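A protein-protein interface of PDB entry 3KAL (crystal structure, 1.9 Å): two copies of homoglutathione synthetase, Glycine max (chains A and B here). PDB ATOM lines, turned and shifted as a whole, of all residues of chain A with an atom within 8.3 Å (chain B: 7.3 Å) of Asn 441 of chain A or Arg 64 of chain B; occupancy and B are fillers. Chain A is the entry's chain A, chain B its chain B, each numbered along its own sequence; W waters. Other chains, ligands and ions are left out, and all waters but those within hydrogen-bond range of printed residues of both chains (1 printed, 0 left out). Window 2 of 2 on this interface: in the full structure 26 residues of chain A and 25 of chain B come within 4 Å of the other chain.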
ATOM      1  N   VAL A  43     -17.715  33.020   5.075  1.00  0.00           N
ATOM      2  CA  VAL A  43     -17.277  32.003   6.065  1.00  0.00           C
ATOM      3  C   VAL A  43     -17.471  30.578   5.454  1.00  0.00           C
ATOM      4  O   VAL A  43     -16.584  29.728   5.628  1.00  0.00           O
ATOM      5  CB  VAL A  43     -18.047  32.149   7.419  1.00  0.00           C
ATOM      6  CG1 VAL A  43     -17.878  30.841   8.338  1.00  0.00           C
ATOM      7  CG2 VAL A  43     -17.552  33.478   8.141  1.00  0.00           C
ATOM      8  N   LEU A  47     -14.538  27.665   4.809  1.00  0.00           N
ATOM      9  CA  LEU A  47     -14.531  26.350   5.498  1.00  0.00           C
ATOM     10  C   LEU A  47     -14.389  25.262   4.392  1.00  0.00           C
ATOM     11  O   LEU A  47     -13.701  24.213   4.626  1.00  0.00           O
ATOM     12  CB  LEU A  47     -15.771  26.130   6.370  1.00  0.00           C
ATOM     13  CG  LEU A  47     -15.893  27.137   7.585  1.00  0.00           C
ATOM     14  CD1 LEU A  47     -17.240  27.041   8.309  1.00  0.00           C
ATOM     15  CD2 LEU A  47     -14.727  26.953   8.563  1.00  0.00           C
ATOM     16  N   ASP A  59      -7.994  17.735  15.584  1.00  0.00           N
ATOM     17  CA  ASP A  59      -8.795  18.572  16.584  1.00  0.00           C
ATOM     18  C   ASP A  59      -8.310  18.140  18.025  1.00  0.00           C
ATOM     19  O   ASP A  59      -8.249  16.918  18.331  1.00  0.00           O
ATOM     20  CB  ASP A  59     -10.276  18.209  16.283  1.00  0.00           C
ATOM     21  CG  ASP A  59     -11.327  19.021  17.104  1.00  0.00           C
ATOM     22  OD1 ASP A  59     -10.998  19.447  18.181  1.00  0.00           O
ATOM     23  OD2 ASP A  59     -12.418  19.069  16.518  1.00  0.00           O
ATOM     24  N   VAL A  74     -10.043  19.028  11.704  1.00  0.00           N
ATOM     25  CA  VAL A  74     -10.656  20.398  11.814  1.00  0.00           C
ATOM     26  C   VAL A  74      -9.866  21.490  11.079  1.00  0.00           C
ATOM     27  O   VAL A  74      -8.594  21.371  11.005  1.00  0.00           O
ATOM     28  CB  VAL A  74     -10.899  20.702  13.294  1.00  0.00           C
ATOM     29  CG1 VAL A  74      -9.555  20.995  14.052  1.00  0.00           C
ATOM     30  CG2 VAL A  74     -12.038  21.978  13.360  1.00  0.00           C
ATOM     31  N   HIS A  75     -10.517  22.501  10.468  1.00  0.00           N
ATOM     32  CA  HIS A  75      -9.765  23.498   9.801  1.00  0.00           C
ATOM     33  C   HIS A  75      -8.932  24.261  10.860  1.00  0.00           C
ATOM     34  O   HIS A  75      -9.265  24.378  12.120  1.00  0.00           O
ATOM     35  CB  HIS A  75     -10.738  24.490   9.055  1.00  0.00           C
ATOM     36  CG  HIS A  75     -11.516  25.372  10.051  1.00  0.00           C
ATOM     37  ND1 HIS A  75     -11.021  26.564  10.537  1.00  0.00           N
ATOM     38  CD2 HIS A  75     -12.726  25.173  10.682  1.00  0.00           C
ATOM     39  CE1 HIS A  75     -11.859  27.028  11.454  1.00  0.00           C
ATOM     40  NE2 HIS A  75     -12.936  26.258  11.483  1.00  0.00           N
ATOM     41  N   PRO A  77      -7.579  27.236  12.980  1.00  0.00           N
ATOM     42  CA  PRO A  77      -8.172  28.591  13.400  1.00  0.00           C
ATOM     43  C   PRO A  77      -7.583  29.733  12.524  1.00  0.00           C
ATOM     44  O   PRO A  77      -6.333  29.845  12.250  1.00  0.00           O
ATOM     45  CB  PRO A  77      -7.712  28.731  14.851  1.00  0.00           C
ATOM     46  CG  PRO A  77      -7.383  27.309  15.278  1.00  0.00           C
ATOM     47  CD  PRO A  77      -6.777  26.605  14.078  1.00  0.00           C
ATOM     48  N   LEU A  78      -8.474  30.541  11.896  1.00  0.00           N
ATOM     49  CA  LEU A  78      -8.060  31.418  10.863  1.00  0.00           C
ATOM     50  C   LEU A  78      -8.769  32.773  11.047  1.00  0.00           C
ATOM     51  O   LEU A  78      -9.873  32.829  11.601  1.00  0.00           O
ATOM     52  CB  LEU A  78      -8.358  30.780   9.474  1.00  0.00           C
ATOM     53  CG  LEU A  78      -9.786  30.316   8.992  1.00  0.00           C
ATOM     54  CD1 LEU A  78     -10.437  31.644   8.242  1.00  0.00           C
ATOM     55  CD2 LEU A  78      -9.493  29.225   7.947  1.00  0.00           C
ATOM     56  N   ILE A 435     -12.562  39.024  11.345  1.00  0.00           N
ATOM     57  CA  ILE A 435     -13.455  37.879  11.659  1.00  0.00           C
ATOM     58  C   ILE A 435     -12.684  36.617  12.062  1.00  0.00           C
ATOM     59  O   ILE A 435     -11.860  36.165  11.283  1.00  0.00           O
ATOM     60  CB  ILE A 435     -14.449  37.710  10.469  1.00  0.00           C
ATOM     61  CG1 ILE A 435     -15.332  38.993  10.211  1.00  0.00           C
ATOM     62  CG2 ILE A 435     -15.330  36.328  10.741  1.00  0.00           C
ATOM     63  CD1 ILE A 435     -16.247  39.245  11.434  1.00  0.00           C
ATOM     64  N   LEU A 436     -12.793  36.129  13.276  1.00  0.00           N
ATOM     65  CA  LEU A 436     -12.042  34.939  13.742  1.00  0.00           C
ATOM     66  C   LEU A 436     -12.844  33.678  13.610  1.00  0.00           C
ATOM     67  O   LEU A 436     -13.989  33.553  14.117  1.00  0.00           O
ATOM     68  CB  LEU A 436     -11.444  35.116  15.171  1.00  0.00           C
ATOM     69  CG  LEU A 436     -10.658  36.402  15.529  1.00  0.00           C
ATOM     70  CD1 LEU A 436      -9.699  35.990  16.715  1.00  0.00           C
ATOM     71  CD2 LEU A 436      -9.695  36.675  14.524  1.00  0.00           C
ATOM     72  N   VAL A 437     -12.289  32.705  12.850  1.00  0.00           N
ATOM     73  CA  VAL A 437     -13.096  31.448  12.510  1.00  0.00           C
ATOM     74  C   VAL A 437     -12.421  30.306  13.216  1.00  0.00           C
ATOM     75  O   VAL A 437     -11.282  30.073  13.003  1.00  0.00           O
ATOM     76  CB  VAL A 437     -13.269  31.141  11.015  1.00  0.00           C
ATOM     77  CG1 VAL A 437     -14.258  29.858  10.795  1.00  0.00           C
ATOM     78  CG2 VAL A 437     -13.557  32.466  10.130  1.00  0.00           C
ATOM     79  N   ARG A 438     -13.151  29.596  14.069  1.00  0.00           N
ATOM     80  CA  ARG A 438     -12.583  28.628  14.986  1.00  0.00           C
ATOM     81  C   ARG A 438     -13.600  27.527  15.222  1.00  0.00           C
ATOM     82  O   ARG A 438     -14.654  27.745  15.865  1.00  0.00           O
ATOM     83  CB  ARG A 438     -12.241  29.255  16.346  1.00  0.00           C
ATOM     84  CG  ARG A 438     -11.331  30.494  16.497  1.00  0.00           C
ATOM     85  CD  ARG A 438     -10.552  30.543  17.886  1.00  0.00           C
ATOM     86  NE  ARG A 438     -10.058  31.891  18.030  1.00  0.00           N
ATOM     87  CZ  ARG A 438      -9.073  32.344  18.799  1.00  0.00           C
ATOM     88  NH1 ARG A 438      -8.321  31.534  19.524  1.00  0.00           N
ATOM     89  NH2 ARG A 438      -8.811  33.646  18.788  1.00  0.00           N
ATOM     90  N   ASP A 439     -13.278  26.304  14.763  1.00  0.00           N
ATOM     91  CA  ASP A 439     -14.193  25.141  14.773  1.00  0.00           C
ATOM     92  C   ASP A 439     -15.575  25.393  14.087  1.00  0.00           C
ATOM     93  O   ASP A 439     -16.579  24.993  14.638  1.00  0.00           O
ATOM     94  CB  ASP A 439     -14.380  24.644  16.235  1.00  0.00           C
ATOM     95  CG  ASP A 439     -14.865  23.165  16.309  1.00  0.00           C
ATOM     96  OD1 ASP A 439     -15.165  22.749  17.472  1.00  0.00           O
ATOM     97  OD2 ASP A 439     -14.968  22.356  15.278  1.00  0.00           O
ATOM     98  N   GLY A 440     -15.595  26.118  12.971  1.00  0.00           N
ATOM     99  CA  GLY A 440     -16.760  26.232  12.158  1.00  0.00           C
ATOM    100  C   GLY A 440     -17.643  27.453  12.602  1.00  0.00           C
ATOM    101  O   GLY A 440     -18.598  27.755  11.994  1.00  0.00           O
ATOM    102  N   ASN A 441     -17.248  28.109  13.648  1.00  0.00           N
ATOM    103  CA  ASN A 441     -17.946  29.330  14.170  1.00  0.00           C
ATOM    104  C   ASN A 441     -17.096  30.568  13.977  1.00  0.00           C
ATOM    105  O   ASN A 441     -15.911  30.481  14.049  1.00  0.00           O
ATOM    106  CB  ASN A 441     -18.188  29.048  15.604  1.00  0.00           C
ATOM    107  CG  ASN A 441     -19.334  28.050  15.793  1.00  0.00           C
ATOM    108  OD1 ASN A 441     -20.419  28.201  15.179  1.00  0.00           O
ATOM    109  ND2 ASN A 441     -19.054  26.937  16.493  1.00  0.00           N
ATOM    110  N   TRP A 442     -17.691  31.750  13.790  1.00  0.00           N
ATOM    111  CA  TRP A 442     -16.949  32.997  13.577  1.00  0.00           C
ATOM    112  C   TRP A 442     -17.391  34.001  14.698  1.00  0.00           C
ATOM    113  O   TRP A 442     -18.470  33.853  15.343  1.00  0.00           O
ATOM    114  CB  TRP A 442     -17.207  33.516  12.178  1.00  0.00           C
ATOM    115  CG  TRP A 442     -18.691  34.002  11.960  1.00  0.00           C
ATOM    116  CD1 TRP A 442     -19.687  33.289  11.393  1.00  0.00           C
ATOM    117  CD2 TRP A 442     -19.284  35.297  12.302  1.00  0.00           C
ATOM    118  NE1 TRP A 442     -20.842  34.032  11.296  1.00  0.00           N
ATOM    119  CE2 TRP A 442     -20.654  35.255  11.873  1.00  0.00           C
ATOM    120  CE3 TRP A 442     -18.807  36.458  12.893  1.00  0.00           C
ATOM    121  CZ2 TRP A 442     -21.574  36.369  12.043  1.00  0.00           C
ATOM    122  CZ3 TRP A 442     -19.778  37.592  13.131  1.00  0.00           C
ATOM    123  CH2 TRP A 442     -21.105  37.488  12.719  1.00  0.00           C
ATOM    124  N   ASP A 443     -16.457  34.852  15.078  1.00  0.00           N
ATOM    125  CA  ASP A 443     -16.718  35.980  15.983  1.00  0.00           C
ATOM    126  C   ASP A 443     -15.999  37.233  15.495  1.00  0.00           C
ATOM    127  O   ASP A 443     -15.125  37.118  14.676  1.00  0.00           O
ATOM    128  CB  ASP A 443     -16.348  35.575  17.402  1.00  0.00           C
ATOM    129  CG  ASP A 443     -17.147  36.375  18.477  1.00  0.00           C
ATOM    130  OD1 ASP A 443     -17.992  37.349  18.128  1.00  0.00           O
ATOM    131  OD2 ASP A 443     -16.877  36.042  19.682  1.00  0.00           O
ATOM    132  N   THR A 444     -16.415  38.470  15.936  1.00  0.00           N
ATOM    133  CA  THR A 444     -15.666  39.686  15.612  1.00  0.00           C
ATOM    134  C   THR A 444     -14.601  39.817  16.739  1.00  0.00           C
ATOM    135  O   THR A 444     -14.738  39.262  17.898  1.00  0.00           O
ATOM    136  CB  THR A 444     -16.686  40.950  15.572  1.00  0.00           C
ATOM    137  OG1 THR A 444     -17.269  40.852  16.836  1.00  0.00           O
ATOM    138  CG2 THR A 444     -17.731  40.757  14.485  1.00  0.00           C
ATOM    139  N   GLY B  58     -17.829  14.305   6.144  1.00  0.00           N
ATOM    140  CA  GLY B  58     -18.286  14.627   7.451  1.00  0.00           C
ATOM    141  C   GLY B  58     -18.349  13.321   8.278  1.00  0.00           C
ATOM    142  O   GLY B  58     -18.887  12.379   7.764  1.00  0.00           O
ATOM    143  N   ASP B  59     -17.832  13.278   9.512  1.00  0.00           N
ATOM    144  CA  ASP B  59     -18.040  12.015  10.408  1.00  0.00           C
ATOM    145  C   ASP B  59     -19.507  12.011  10.995  1.00  0.00           C
ATOM    146  O   ASP B  59     -19.947  12.990  11.598  1.00  0.00           O
ATOM    147  CB  ASP B  59     -16.938  12.152  11.510  1.00  0.00           C
ATOM    148  CG  ASP B  59     -16.852  10.912  12.469  1.00  0.00           C
ATOM    149  OD1 ASP B  59     -17.826  10.256  12.639  1.00  0.00           O
ATOM    150  OD2 ASP B  59     -15.797  10.759  12.964  1.00  0.00           O
ATOM    151  N   LYS B  60     -20.235  10.934  10.748  1.00  0.00           N
ATOM    152  CA  LYS B  60     -21.623  10.668  11.164  1.00  0.00           C
ATOM    153  C   LYS B  60     -21.805  10.886  12.691  1.00  0.00           C
ATOM    154  O   LYS B  60     -22.869  11.284  13.132  1.00  0.00           O
ATOM    155  CB  LYS B  60     -22.109   9.267  10.693  1.00  0.00           C
ATOM    156  CG  LYS B  60     -21.358   8.056  11.411  1.00  0.00           C
ATOM    157  CD  LYS B  60     -21.844   6.691  10.872  1.00  0.00           C
ATOM    158  CE  LYS B  60     -20.958   6.287   9.750  1.00  0.00           C
ATOM    159  NZ  LYS B  60     -21.632   5.366   8.863  1.00  0.00           N
ATOM    160  N   SER B  61     -20.736  10.716  13.456  1.00  0.00           N
ATOM    161  CA  SER B  61     -20.759  10.952  14.899  1.00  0.00           C
ATOM    162  C   SER B  61     -20.616  12.413  15.376  1.00  0.00           C
ATOM    163  O   SER B  61     -20.737  12.677  16.567  1.00  0.00           O
ATOM    164  CB  SER B  61     -19.780  10.002  15.616  1.00  0.00           C
ATOM    165  OG  SER B  61     -18.485  10.534  15.697  1.00  0.00           O
ATOM    166  N   VAL B  62     -20.418  13.362  14.460  1.00  0.00           N
ATOM    167  CA  VAL B  62     -20.149  14.767  14.829  1.00  0.00           C
ATOM    168  C   VAL B  62     -21.379  15.469  14.275  1.00  0.00           C
ATOM    169  O   VAL B  62     -21.764  15.331  13.065  1.00  0.00           O
ATOM    170  CB  VAL B  62     -18.807  15.264  14.168  1.00  0.00           C
ATOM    171  CG1 VAL B  62     -18.544  16.664  14.557  1.00  0.00           C
ATOM    172  CG2 VAL B  62     -17.666  14.406  14.547  1.00  0.00           C
ATOM    173  N   GLN B  63     -22.153  16.073  15.193  1.00  0.00           N
ATOM    174  CA  GLN B  63     -23.590  16.423  14.750  1.00  0.00           C
ATOM    175  C   GLN B  63     -23.719  17.348  13.445  1.00  0.00           C
ATOM    176  O   GLN B  63     -24.578  17.059  12.543  1.00  0.00           O
ATOM    177  CB  GLN B  63     -24.433  17.088  15.929  1.00  0.00           C
ATOM    178  CG  GLN B  63     -25.967  16.746  15.882  1.00  0.00           C
ATOM    179  CD  GLN B  63     -26.673  16.933  14.466  1.00  0.00           C
ATOM    180  OE1 GLN B  63     -26.888  15.938  13.678  1.00  0.00           O
ATOM    181  NE2 GLN B  63     -27.047  18.213  14.160  1.00  0.00           N
ATOM    182  N   ARG B  64     -22.900  18.402  13.405  1.00  0.00           N
ATOM    183  CA  ARG B  64     -22.963  19.445  12.345  1.00  0.00           C
ATOM    184  C   ARG B  64     -22.126  19.139  11.067  1.00  0.00           C
ATOM    185  O   ARG B  64     -21.984  20.018  10.182  1.00  0.00           O
ATOM    186  CB  ARG B  64     -22.673  20.857  12.870  1.00  0.00           C
ATOM    187  CG  ARG B  64     -21.559  21.070  13.821  1.00  0.00           C
ATOM    188  CD  ARG B  64     -21.821  22.259  14.703  1.00  0.00           C
ATOM    189  NE  ARG B  64     -21.276  23.502  14.205  1.00  0.00           N
ATOM    190  CZ  ARG B  64     -19.962  23.808  14.222  1.00  0.00           C
ATOM    191  NH1 ARG B  64     -19.021  22.927  14.649  1.00  0.00           N
ATOM    192  NH2 ARG B  64     -19.572  24.970  13.758  1.00  0.00           N
ATOM    193  N   SER B  65     -21.563  17.930  10.996  1.00  0.00           N
ATOM    194  CA  SER B  65     -20.525  17.630   9.946  1.00  0.00           C
ATOM    195  C   SER B  65     -21.198  17.492   8.551  1.00  0.00           C
ATOM    196  O   SER B  65     -20.500  17.439   7.553  1.00  0.00           O
ATOM    197  CB  SER B  65     -19.758  16.316  10.238  1.00  0.00           C
ATOM    198  OG  SER B  65     -20.637  15.172   9.945  1.00  0.00           O
ATOM    199  N   GLY B  66     -22.517  17.401   8.504  1.00  0.00           N
ATOM    200  CA  GLY B  66     -23.196  17.266   7.242  1.00  0.00           C
ATOM    201  C   GLY B  66     -23.778  18.676   6.850  1.00  0.00           C
ATOM    202  O   GLY B  66     -24.425  18.794   5.812  1.00  0.00           O
ATOM    203  N   ARG B  67     -23.541  19.704   7.686  1.00  0.00           N
ATOM    204  CA  ARG B  67     -23.965  21.159   7.432  1.00  0.00           C
ATOM    205  C   ARG B  67     -22.834  22.176   7.308  1.00  0.00           C
ATOM    206  O   ARG B  67     -22.856  23.049   6.426  1.00  0.00           O
ATOM    207  CB  ARG B  67     -24.833  21.757   8.570  1.00  0.00           C
ATOM    208  CG  ARG B  67     -25.894  20.890   9.271  1.00  0.00           C
ATOM    209  CD  ARG B  67     -26.916  21.740  10.171  1.00  0.00           C
ATOM    210  NE  ARG B  67     -26.293  22.361  11.374  1.00  0.00           N
ATOM    211  CZ  ARG B  67     -25.906  23.639  11.489  1.00  0.00           C
ATOM    212  NH1 ARG B  67     -26.095  24.497  10.481  1.00  0.00           N
ATOM    213  NH2 ARG B  67     -25.371  24.075  12.633  1.00  0.00           N
ATOM    214  N   VAL B  68     -21.923  22.127   8.271  1.00  0.00           N
ATOM    215  CA  VAL B  68     -20.890  23.112   8.483  1.00  0.00           C
ATOM    216  C   VAL B  68     -19.610  22.465   7.892  1.00  0.00           C
ATOM    217  O   VAL B  68     -19.213  21.408   8.495  1.00  0.00           O
ATOM    218  CB  VAL B  68     -20.731  23.311   9.989  1.00  0.00           C
ATOM    219  CG1 VAL B  68     -19.664  24.311  10.178  1.00  0.00           C
ATOM    220  CG2 VAL B  68     -22.131  23.888  10.613  1.00  0.00           C
ATOM    221  N   PRO B  69     -19.034  23.011   6.768  1.00  0.00           N
ATOM    222  CA  PRO B  69     -17.798  22.456   6.140  1.00  0.00           C
ATOM    223  C   PRO B  69     -16.640  22.654   7.236  1.00  0.00           C
ATOM    224  O   PRO B  69     -16.648  23.613   8.018  1.00  0.00           O
ATOM    225  CB  PRO B  69     -17.586  23.339   4.915  1.00  0.00           C
ATOM    226  CG  PRO B  69     -19.066  24.064   4.764  1.00  0.00           C
ATOM    227  CD  PRO B  69     -19.396  24.280   6.139  1.00  0.00           C
ATOM    228  N   GLY B  70     -15.607  21.754   7.297  1.00  0.00           N
ATOM    229  CA  GLY B  70     -14.390  22.129   7.973  1.00  0.00           C
ATOM    230  C   GLY B  70     -14.288  21.517   9.271  1.00  0.00           C
ATOM    231  O   GLY B  70     -13.345  21.843  10.026  1.00  0.00           O
ATOM    232  N   VAL B  71     -15.344  20.858   9.638  1.00  0.00           N
ATOM    233  CA  VAL B  71     -15.456  20.408  10.993  1.00  0.00           C
ATOM    234  C   VAL B  71     -15.915  18.908  11.049  1.00  0.00           C
ATOM    235  O   VAL B  71     -16.719  18.376  10.217  1.00  0.00           O
ATOM    236  CB  VAL B  71     -16.457  21.305  11.954  1.00  0.00           C
ATOM    237  CG1 VAL B  71     -16.167  22.721  11.903  1.00  0.00           C
ATOM    238  CG2 VAL B  71     -17.990  20.956  11.551  1.00  0.00           C
ATOM    239  N   GLY B  72     -15.361  18.218  12.050  1.00  0.00           N
ATOM    240  CA  GLY B  72     -15.670  16.821  12.241  1.00  0.00           C
ATOM    241  C   GLY B  72     -15.391  15.979  10.972  1.00  0.00           C
ATOM    242  O   GLY B  72     -16.261  15.224  10.464  1.00  0.00           O
ATOM    243  N   GLU B 240     -28.758  17.515   4.526  1.00  0.00           N
ATOM    244  CA  GLU B 240     -27.502  17.085   5.234  1.00  0.00           C
ATOM    245  C   GLU B 240     -26.736  16.302   4.224  1.00  0.00           C
ATOM    246  O   GLU B 240     -27.294  15.513   3.481  1.00  0.00           O
ATOM    247  CB  GLU B 240     -27.807  16.267   6.516  1.00  0.00           C
ATOM    248  CG  GLU B 240     -27.073  17.001   7.938  1.00  0.00           C
ATOM    249  CD  GLU B 240     -28.263  17.353   8.598  1.00  0.00           C
ATOM    250  OE1 GLU B 240     -29.164  16.715   7.970  1.00  0.00           O
ATOM    251  OE2 GLU B 240     -28.415  18.253   9.443  1.00  0.00           O
ATOM    252  N   ARG B 242     -23.044  14.884   4.246  1.00  0.00           N
ATOM    253  CA  ARG B 242     -21.651  14.526   4.647  1.00  0.00           C
ATOM    254  C   ARG B 242     -20.652  14.320   3.563  1.00  0.00           C
ATOM    255  O   ARG B 242     -19.453  14.507   3.809  1.00  0.00           O
ATOM    256  CB  ARG B 242     -21.625  13.302   5.699  1.00  0.00           C
ATOM    257  CG  ARG B 242     -22.176  13.759   6.989  1.00  0.00           C
ATOM    258  CD  ARG B 242     -22.177  12.534   8.062  1.00  0.00           C
ATOM    259  NE  ARG B 242     -22.566  11.208   7.554  1.00  0.00           N
ATOM    260  CZ  ARG B 242     -21.794  10.131   7.232  1.00  0.00           C
ATOM    261  NH1 ARG B 242     -22.466   9.061   6.803  1.00  0.00           N
ATOM    262  NH2 ARG B 242     -20.395  10.068   7.207  1.00  0.00           N
ATOM    263  N   MET B 244     -20.372  16.310   1.021  1.00  0.00           N
ATOM    264  CA  MET B 244     -20.488  17.631   0.353  1.00  0.00           C
ATOM    265  C   MET B 244     -19.224  17.973  -0.361  1.00  0.00           C
ATOM    266  O   MET B 244     -19.203  18.840  -1.326  1.00  0.00           O
ATOM    267  CB  MET B 244     -20.963  18.697   1.405  1.00  0.00           C
ATOM    268  CG  MET B 244     -19.781  19.010   2.530  1.00  0.00           C
ATOM    269  SD  MET B 244     -19.861  20.466   3.520  1.00  0.00           S
ATOM    270  CE  MET B 244     -21.190  19.975   4.492  1.00  0.00           C
ATOM    271  N   TYR B 245     -18.061  17.484   0.144  1.00  0.00           N
ATOM    272  CA  TYR B 245     -16.759  17.859  -0.457  1.00  0.00           C
ATOM    273  C   TYR B 245     -16.611  17.499  -1.908  1.00  0.00           C
ATOM    274  O   TYR B 245     -16.103  18.266  -2.720  1.00  0.00           O
ATOM    275  CB  TYR B 245     -15.542  17.375   0.409  1.00  0.00           C
ATOM    276  CG  TYR B 245     -15.801  17.944   1.779  1.00  0.00           C
ATOM    277  CD1 TYR B 245     -16.290  17.078   2.848  1.00  0.00           C
ATOM    278  CD2 TYR B 245     -15.729  19.456   2.022  1.00  0.00           C
ATOM    279  CE1 TYR B 245     -16.582  17.613   4.155  1.00  0.00           C
ATOM    280  CE2 TYR B 245     -16.068  19.950   3.299  1.00  0.00           C
ATOM    281  CZ  TYR B 245     -16.484  19.003   4.285  1.00  0.00           C
ATOM    282  OH  TYR B 245     -16.749  19.490   5.451  1.00  0.00           O
HETATM  283  O   HOH W   1     -21.742  26.229  13.475  1.00  0.00           O
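Water W1 bridges NH2 of Arg 64 of chain B (2.5 Å) and OD1 of Asn 441 of chain A (2.9 Å).
Among the printed residues, pairs that only touch across the chains: Leu 47 of chain A with Pro 69 of chain B, Asp 439 of chain A with Val 71 of chain B, Val 74 of chain A with Gly 70 of chain B and Gly 440 of chain A with Val 71 of chain B.
The side-chain hydroxyl (OH) of Tyr 245 of chain B is in hydrogen-bond range of the backbone NH (N) of Gly 70 of chain B, 3.1 Å away. A ring nitrogen (NE2) of His 75 of chain A lies within hydrogen-bond range of the backbone NH (N) of Asp 439 of chain A (3.3 Å). N of Gly 440 of chain A sits at hydrogen-bond distance from NE2 of His 75 of chain A (3.1 Å).
1 position is printed for both chains. Of the 8 pairs that touch across the chains among the printed residues, none has its exchanged pair printed and touching as well.
Of the printed residues of chain B, Leu 47 of chain A touches Pro 69 (3.1 Å). Of the printed residues of chain B, His 75 of chain A touches Gly 70 (2.9 Å). Of the printed residues of chain B, Gly 440 of chain A touches Arg 64 and Val 71. Of the printed residues of chain B, Asn 441 of chain A touches Arg 64 (3.4 Å). Of the printed residues of chain A, Arg 64 of chain B touches Asp 439, Gly 440 and Asn 441. Printed residues of chain A within 4 Å of Gly 70 of chain B: Val 74 (3.5 Å) and His 75 (2.9 Å). Printed residues of chain A within 4 Å of Val 71 of chain B: Asp 439 and Gly 440. Arg 242 of chain B touches none of the printed residues of chain A. The nearest printed residue of chain B that does not touch Asn 441 of chain A is Val 68 of chain B (5.7 Å). The nearest printed residue of chain A that does not touch Arg 64 of chain B is Arg 438 of chain A (6.0 Å).
The guanidinium group (NH2) of Arg 64 of chain B lies within hydrogen-bond range of the backbone carbonyl oxygen (O) of Asp 439 of chain A (3.1 Å). The guanidinium group (NH2) of Arg 64 of chain B lies close to the side-chain amide nitrogen (ND2) of Asn 441 of chain A. NH2 of Arg 64 of chain B lies close to O of Gly 440 of chain A. O of Gly 70 of chain B sits at hydrogen-bond distance from N of His 75 of chain A, 2.9 Å away.
Hydrophobic or aromatic side chains of chain B that line the printed part of chain A: Pro 69 and Val 71. Of the 17 printed residues of chain A, 6 touch a printed residue of chain B. Among the printed residues, 8 pairs touch across the chains.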
